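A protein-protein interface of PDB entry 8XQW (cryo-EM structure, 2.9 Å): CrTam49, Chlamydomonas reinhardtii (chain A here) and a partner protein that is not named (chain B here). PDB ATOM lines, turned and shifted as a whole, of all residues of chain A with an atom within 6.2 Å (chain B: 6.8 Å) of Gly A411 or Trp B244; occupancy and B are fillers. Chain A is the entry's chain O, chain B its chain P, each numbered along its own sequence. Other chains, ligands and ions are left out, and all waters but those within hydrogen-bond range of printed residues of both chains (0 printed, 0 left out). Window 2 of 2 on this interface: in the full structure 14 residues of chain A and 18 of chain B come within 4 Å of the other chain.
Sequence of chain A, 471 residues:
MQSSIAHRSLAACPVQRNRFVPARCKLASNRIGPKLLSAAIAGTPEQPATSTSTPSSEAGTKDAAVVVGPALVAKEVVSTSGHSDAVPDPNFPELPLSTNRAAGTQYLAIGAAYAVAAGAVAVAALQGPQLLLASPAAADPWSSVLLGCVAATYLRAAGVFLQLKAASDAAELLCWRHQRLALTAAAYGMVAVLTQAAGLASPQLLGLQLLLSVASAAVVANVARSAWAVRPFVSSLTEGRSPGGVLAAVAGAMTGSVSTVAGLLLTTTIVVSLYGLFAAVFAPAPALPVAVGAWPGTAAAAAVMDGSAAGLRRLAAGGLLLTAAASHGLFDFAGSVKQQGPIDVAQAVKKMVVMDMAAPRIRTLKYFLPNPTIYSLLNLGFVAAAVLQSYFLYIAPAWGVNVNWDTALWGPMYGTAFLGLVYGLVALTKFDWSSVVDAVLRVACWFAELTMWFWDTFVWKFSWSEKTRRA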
ATOM      1  N   VAL A 272     -32.772  -9.458  -6.064  1.00  0.00           N
ATOM      2  CA  VAL A 272     -32.495  -9.393  -4.630  1.00  0.00           C
ATOM      3  C   VAL A 272     -33.570  -8.585  -3.915  1.00  0.00           C
ATOM      4  O   VAL A 272     -34.043  -8.974  -2.841  1.00  0.00           O
ATOM      5  CB  VAL A 272     -31.078  -8.840  -4.350  1.00  0.00           C
ATOM      6  CG1 VAL A 272     -30.971  -7.349  -4.637  1.00  0.00           C
ATOM      7  CG2 VAL A 272     -30.689  -9.102  -2.903  1.00  0.00           C
ATOM      8  N   VAL A 403     -27.059  -5.443  13.723  1.00  0.00           N
ATOM      9  CA  VAL A 403     -27.487  -5.611  12.346  1.00  0.00           C
ATOM     10  C   VAL A 403     -27.421  -7.076  11.919  1.00  0.00           C
ATOM     11  O   VAL A 403     -27.888  -7.430  10.841  1.00  0.00           O
ATOM     12  CB  VAL A 403     -26.661  -4.722  11.404  1.00  0.00           C
ATOM     13  CG1 VAL A 403     -26.445  -3.359  12.023  1.00  0.00           C
ATOM     14  CG2 VAL A 403     -25.331  -5.376  11.089  1.00  0.00           C
ATOM     15  N   ASN A 404     -26.861  -7.940  12.762  1.00  0.00           N
ATOM     16  CA  ASN A 404     -26.512  -9.294  12.358  1.00  0.00           C
ATOM     17  C   ASN A 404     -27.541 -10.346  12.734  1.00  0.00           C
ATOM     18  O   ASN A 404     -27.588 -11.394  12.093  1.00  0.00           O
ATOM     19  CB  ASN A 404     -25.161  -9.694  12.963  1.00  0.00           C
ATOM     20  CG  ASN A 404     -23.994  -8.962  12.326  1.00  0.00           C
ATOM     21  OD1 ASN A 404     -23.894  -8.868  11.107  1.00  0.00           O
ATOM     22  ND2 ASN A 404     -23.103  -8.440  13.156  1.00  0.00           N
ATOM     23  N   ASP A 406     -30.826 -10.363  12.493  1.00  0.00           N
ATOM     24  CA  ASP A 406     -31.943 -10.468  11.564  1.00  0.00           C
ATOM     25  C   ASP A 406     -31.457 -10.259  10.137  1.00  0.00           C
ATOM     26  O   ASP A 406     -31.182  -9.125   9.729  1.00  0.00           O
ATOM     27  CB  ASP A 406     -33.034  -9.451  11.893  1.00  0.00           C
ATOM     28  CG  ASP A 406     -34.115  -9.402  10.834  1.00  0.00           C
ATOM     29  OD1 ASP A 406     -33.943  -8.660   9.846  1.00  0.00           O
ATOM     30  OD2 ASP A 406     -35.134 -10.106  10.984  1.00  0.00           O
ATOM     31  N   THR A 407     -31.387 -11.347   9.376  1.00  0.00           N
ATOM     32  CA  THR A 407     -30.948 -11.298   7.989  1.00  0.00           C
ATOM     33  C   THR A 407     -32.026 -10.805   7.037  1.00  0.00           C
ATOM     34  O   THR A 407     -31.698 -10.252   5.982  1.00  0.00           O
ATOM     35  CB  THR A 407     -30.499 -12.685   7.527  1.00  0.00           C
ATOM     36  OG1 THR A 407     -31.632 -13.413   7.041  1.00  0.00           O
ATOM     37  CG2 THR A 407     -29.877 -13.447   8.682  1.00  0.00           C
ATOM     38  N   ALA A 408     -33.297 -10.994   7.383  1.00  0.00           N
ATOM     39  CA  ALA A 408     -34.411 -10.702   6.490  1.00  0.00           C
ATOM     40  C   ALA A 408     -34.595  -9.218   6.225  1.00  0.00           C
ATOM     41  O   ALA A 408     -35.410  -8.860   5.372  1.00  0.00           O
ATOM     42  CB  ALA A 408     -35.703 -11.287   7.058  1.00  0.00           C
ATOM     43  N   LEU A 409     -33.874  -8.349   6.926  1.00  0.00           N
ATOM     44  CA  LEU A 409     -33.982  -6.915   6.702  1.00  0.00           C
ATOM     45  C   LEU A 409     -32.682  -6.291   6.223  1.00  0.00           C
ATOM     46  O   LEU A 409     -32.673  -5.619   5.186  1.00  0.00           O
ATOM     47  CB  LEU A 409     -34.447  -6.213   7.984  1.00  0.00           C
ATOM     48  CG  LEU A 409     -34.448  -4.694   7.884  1.00  0.00           C
ATOM     49  CD1 LEU A 409     -35.482  -4.278   6.871  1.00  0.00           C
ATOM     50  CD2 LEU A 409     -34.723  -4.061   9.234  1.00  0.00           C
ATOM     51  N   TRP A 410     -31.578  -6.495   6.943  1.00  0.00           N
ATOM     52  CA  TRP A 410     -30.329  -5.814   6.625  1.00  0.00           C
ATOM     53  C   TRP A 410     -29.632  -6.376   5.399  1.00  0.00           C
ATOM     54  O   TRP A 410     -28.880  -5.647   4.742  1.00  0.00           O
ATOM     55  CB  TRP A 410     -29.372  -5.883   7.815  1.00  0.00           C
ATOM     56  CG  TRP A 410     -29.973  -5.401   9.084  1.00  0.00           C
ATOM     57  CD1 TRP A 410     -30.629  -6.147  10.015  1.00  0.00           C
ATOM     58  CD2 TRP A 410     -29.982  -4.057   9.566  1.00  0.00           C
ATOM     59  NE1 TRP A 410     -31.041  -5.350  11.052  1.00  0.00           N
ATOM     60  CE2 TRP A 410     -30.656  -4.060  10.797  1.00  0.00           C
ATOM     61  CE3 TRP A 410     -29.480  -2.850   9.076  1.00  0.00           C
ATOM     62  CZ2 TRP A 410     -30.844  -2.903  11.544  1.00  0.00           C
ATOM     63  CZ3 TRP A 410     -29.671  -1.707   9.815  1.00  0.00           C
ATOM     64  CH2 TRP A 410     -30.342  -1.740  11.035  1.00  0.00           C
ATOM     65  N   GLY A 411     -29.848  -7.647   5.089  1.00  0.00           N
ATOM     66  CA  GLY A 411     -29.239  -8.272   3.945  1.00  0.00           C
ATOM     67  C   GLY A 411     -29.495  -7.522   2.655  1.00  0.00           C
ATOM     68  O   GLY A 411     -28.562  -7.116   1.955  1.00  0.00           O
ATOM     69  N   PRO A 412     -30.771  -7.373   2.290  1.00  0.00           N
ATOM     70  CA  PRO A 412     -31.087  -6.628   1.063  1.00  0.00           C
ATOM     71  C   PRO A 412     -30.534  -5.219   1.057  1.00  0.00           C
ATOM     72  O   PRO A 412     -30.038  -4.767   0.022  1.00  0.00           O
ATOM     73  CB  PRO A 412     -32.618  -6.645   1.043  1.00  0.00           C
ATOM     74  CG  PRO A 412     -32.966  -7.912   1.735  1.00  0.00           C
ATOM     75  CD  PRO A 412     -31.949  -8.080   2.823  1.00  0.00           C
ATOM     76  N   MET A 413     -30.577  -4.519   2.189  1.00  0.00           N
ATOM     77  CA  MET A 413     -30.067  -3.152   2.232  1.00  0.00           C
ATOM     78  C   MET A 413     -28.577  -3.107   1.924  1.00  0.00           C
ATOM     79  O   MET A 413     -28.133  -2.349   1.051  1.00  0.00           O
ATOM     80  CB  MET A 413     -30.348  -2.542   3.600  1.00  0.00           C
ATOM     81  CG  MET A 413     -31.776  -2.719   4.081  1.00  0.00           C
ATOM     82  SD  MET A 413     -31.849  -2.665   5.874  1.00  0.00           S
ATOM     83  CE  MET A 413     -30.557  -1.470   6.193  1.00  0.00           C
ATOM     84  N   TYR A 414     -27.787  -3.917   2.639  1.00  0.00           N
ATOM     85  CA  TYR A 414     -26.345  -3.958   2.412  1.00  0.00           C
ATOM     86  C   TYR A 414     -26.021  -4.387   0.989  1.00  0.00           C
ATOM     87  O   TYR A 414     -25.178  -3.778   0.317  1.00  0.00           O
ATOM     88  CB  TYR A 414     -25.689  -4.911   3.407  1.00  0.00           C
ATOM     89  CG  TYR A 414     -25.446  -4.325   4.772  1.00  0.00           C
ATOM     90  CD1 TYR A 414     -24.358  -3.504   5.008  1.00  0.00           C
ATOM     91  CD2 TYR A 414     -26.297  -4.606   5.829  1.00  0.00           C
ATOM     92  CE1 TYR A 414     -24.126  -2.972   6.253  1.00  0.00           C
ATOM     93  CE2 TYR A 414     -26.074  -4.076   7.080  1.00  0.00           C
ATOM     94  CZ  TYR A 414     -24.988  -3.259   7.286  1.00  0.00           C
ATOM     95  OH  TYR A 414     -24.758  -2.726   8.531  1.00  0.00           O
ATOM     96  N   GLY A 415     -26.675  -5.451   0.515  1.00  0.00           N
ATOM     97  CA  GLY A 415     -26.381  -5.957  -0.813  1.00  0.00           C
ATOM     98  C   GLY A 415     -26.719  -4.956  -1.897  1.00  0.00           C
ATOM     99  O   GLY A 415     -25.969  -4.784  -2.857  1.00  0.00           O
ATOM    100  N   THR A 416     -27.846  -4.261  -1.742  1.00  0.00           N
ATOM    101  CA  THR A 416     -28.253  -3.281  -2.735  1.00  0.00           C
ATOM    102  C   THR A 416     -27.353  -2.056  -2.703  1.00  0.00           C
ATOM    103  O   THR A 416     -27.052  -1.480  -3.752  1.00  0.00           O
ATOM    104  CB  THR A 416     -29.705  -2.891  -2.500  1.00  0.00           C
ATOM    105  OG1 THR A 416     -30.331  -2.641  -3.763  1.00  0.00           O
ATOM    106  CG2 THR A 416     -29.786  -1.640  -1.648  1.00  0.00           C
ATOM    107  N   PRO B 241     -18.305  -7.113  14.443  1.00  0.00           N
ATOM    108  CA  PRO B 241     -18.258  -7.472  13.023  1.00  0.00           C
ATOM    109  C   PRO B 241     -19.650  -7.629  12.436  1.00  0.00           C
ATOM    110  O   PRO B 241     -20.604  -7.998  13.124  1.00  0.00           O
ATOM    111  CB  PRO B 241     -17.513  -8.807  13.033  1.00  0.00           C
ATOM    112  CG  PRO B 241     -17.926  -9.417  14.323  1.00  0.00           C
ATOM    113  CD  PRO B 241     -18.080  -8.284  15.307  1.00  0.00           C
ATOM    114  N   THR B 242     -19.758  -7.347  11.141  1.00  0.00           N
ATOM    115  CA  THR B 242     -21.025  -7.417  10.427  1.00  0.00           C
ATOM    116  C   THR B 242     -21.000  -8.565   9.431  1.00  0.00           C
ATOM    117  O   THR B 242     -20.071  -8.677   8.629  1.00  0.00           O
ATOM    118  CB  THR B 242     -21.311  -6.107   9.698  1.00  0.00           C
ATOM    119  OG1 THR B 242     -20.349  -5.923   8.654  1.00  0.00           O
ATOM    120  CG2 THR B 242     -21.227  -4.951  10.661  1.00  0.00           C
ATOM    121  N   ARG B 243     -22.037  -9.402   9.475  1.00  0.00           N
ATOM    122  CA  ARG B 243     -22.146 -10.509   8.532  1.00  0.00           C
ATOM    123  C   ARG B 243     -22.058 -10.027   7.090  1.00  0.00           C
ATOM    124  O   ARG B 243     -21.551 -10.738   6.217  1.00  0.00           O
ATOM    125  CB  ARG B 243     -23.467 -11.242   8.753  1.00  0.00           C
ATOM    126  CG  ARG B 243     -23.616 -11.840  10.132  1.00  0.00           C
ATOM    127  CD  ARG B 243     -24.950 -12.532  10.277  1.00  0.00           C
ATOM    128  NE  ARG B 243     -25.417 -13.061   9.004  1.00  0.00           N
ATOM    129  CZ  ARG B 243     -26.071 -14.206   8.874  1.00  0.00           C
ATOM    130  NH1 ARG B 243     -26.341 -14.944   9.942  1.00  0.00           N
ATOM    131  NH2 ARG B 243     -26.458 -14.615   7.676  1.00  0.00           N
ATOM    132  N   TRP B 244     -22.521  -8.805   6.829  1.00  0.00           N
ATOM    133  CA  TRP B 244     -22.845  -8.409   5.464  1.00  0.00           C
ATOM    134  C   TRP B 244     -21.646  -7.820   4.741  1.00  0.00           C
ATOM    135  O   TRP B 244     -21.611  -7.804   3.506  1.00  0.00           O
ATOM    136  CB  TRP B 244     -24.016  -7.439   5.495  1.00  0.00           C
ATOM    137  CG  TRP B 244     -25.110  -8.003   6.314  1.00  0.00           C
ATOM    138  CD1 TRP B 244     -25.540  -7.560   7.522  1.00  0.00           C
ATOM    139  CD2 TRP B 244     -25.886  -9.160   6.007  1.00  0.00           C
ATOM    140  NE1 TRP B 244     -26.555  -8.358   7.981  1.00  0.00           N
ATOM    141  CE2 TRP B 244     -26.785  -9.349   7.064  1.00  0.00           C
ATOM    142  CE3 TRP B 244     -25.914 -10.047   4.931  1.00  0.00           C
ATOM    143  CZ2 TRP B 244     -27.699 -10.387   7.080  1.00  0.00           C
ATOM    144  CZ3 TRP B 244     -26.822 -11.074   4.949  1.00  0.00           C
ATOM    145  CH2 TRP B 244     -27.702 -11.239   6.013  1.00  0.00           C
ATOM    146  N   LEU B 245     -20.661  -7.322   5.475  1.00  0.00           N
ATOM    147  CA  LEU B 245     -19.354  -7.140   4.870  1.00  0.00           C
ATOM    148  C   LEU B 245     -18.769  -8.510   4.562  1.00  0.00           C
ATOM    149  O   LEU B 245     -19.224  -9.529   5.090  1.00  0.00           O
ATOM    150  CB  LEU B 245     -18.428  -6.357   5.793  1.00  0.00           C
ATOM    151  CG  LEU B 245     -18.081  -4.955   5.299  1.00  0.00           C
ATOM    152  CD1 LEU B 245     -17.054  -4.311   6.206  1.00  0.00           C
ATOM    153  CD2 LEU B 245     -17.585  -5.003   3.867  1.00  0.00           C
ATOM    154  N   LEU B 246     -17.767  -8.543   3.693  1.00  0.00           N
ATOM    155  CA  LEU B 246     -17.214  -9.827   3.273  1.00  0.00           C
ATOM    156  C   LEU B 246     -16.600 -10.509   4.488  1.00  0.00           C
ATOM    157  O   LEU B 246     -15.604 -10.049   5.047  1.00  0.00           O
ATOM    158  CB  LEU B 246     -16.211  -9.643   2.139  1.00  0.00           C
ATOM    159  CG  LEU B 246     -14.929  -8.828   2.299  1.00  0.00           C
ATOM    160  CD1 LEU B 246     -13.738  -9.754   2.421  1.00  0.00           C
ATOM    161  CD2 LEU B 246     -14.754  -7.896   1.119  1.00  0.00           C
ATOM    162  N   GLY B 247     -17.236 -11.590   4.932  1.00  0.00           N
ATOM    163  CA  GLY B 247     -16.767 -12.343   6.076  1.00  0.00           C
ATOM    164  C   GLY B 247     -16.849 -11.631   7.404  1.00  0.00           C
ATOM    165  O   GLY B 247     -16.695 -12.272   8.446  1.00  0.00           O
ATOM    166  N   GLY B 248     -17.108 -10.329   7.409  1.00  0.00           N
ATOM    167  CA  GLY B 248     -17.112  -9.598   8.657  1.00  0.00           C
ATOM    168  C   GLY B 248     -15.745  -9.385   9.251  1.00  0.00           C
ATOM    169  O   GLY B 248     -15.604  -9.364  10.475  1.00  0.00           O
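Of the printed residues of chain B, Asn A404 touches Pro B241, Thr B242 and Arg B243.
Printed residues of chain B within 4 Å of Thr A407: Arg B243 (3.8 Å) and Trp B244 (3.5 Å).
Of chain B, only Trp B244 comes within 4 Å of Gly A411.
Printed residues of chain B within 4 Å of Tyr A414: Trp B244 (3.5 Å).
Printed residues of chain A within 4 Å of Thr B242: Asn A404.
The nearest residue of chain A that does not touch Trp B244 is Asn A404 (4.1 Å).
The side-chain amide oxygen (OD1) of Asn A404 is in hydrogen-bond range of the backbone NH (N) of Arg B243.
ND2 of Asn A404 is in hydrogen-bond range of O of Pro B241.
NE1 of Trp B244 is in hydrogen-bond range of O of Val A403.
N of Leu B245 sits close to OG1 of Thr B242, at 3.5 Å.
Among the printed residues, pairs that only touch across the chains: Asn A404 with Thr B242, Tyr A414 with Trp B244, Thr A407 with Trp B244, Thr A407 with Arg B243, Trp A410 with Trp B244 and Gly A411 with Trp B244.
Of the 8 printed residues of chain B, 4 touch a printed residue of chain A.
Printed residues of chain B that touch a printed residue of chain A: Pro B241, Thr B242, Arg B243 and Trp B244.
Hydrophobic or aromatic side chains of chain B within 4 Å of the printed part of chain A: Trp B244.
Of the 14 printed residues of chain A, 6 touch a printed residue of chain B.
Printed residues of chain A that touch a printed residue of chain B: Val A403, Asn A404, Thr A407, Trp A410, Gly A411 and Tyr A414.
Hydrophobic or aromatic side chains of chain A that line the printed part of chain B: Trp A410 and Tyr A414.
Among the printed residues, 9 pairs touch across the chains.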
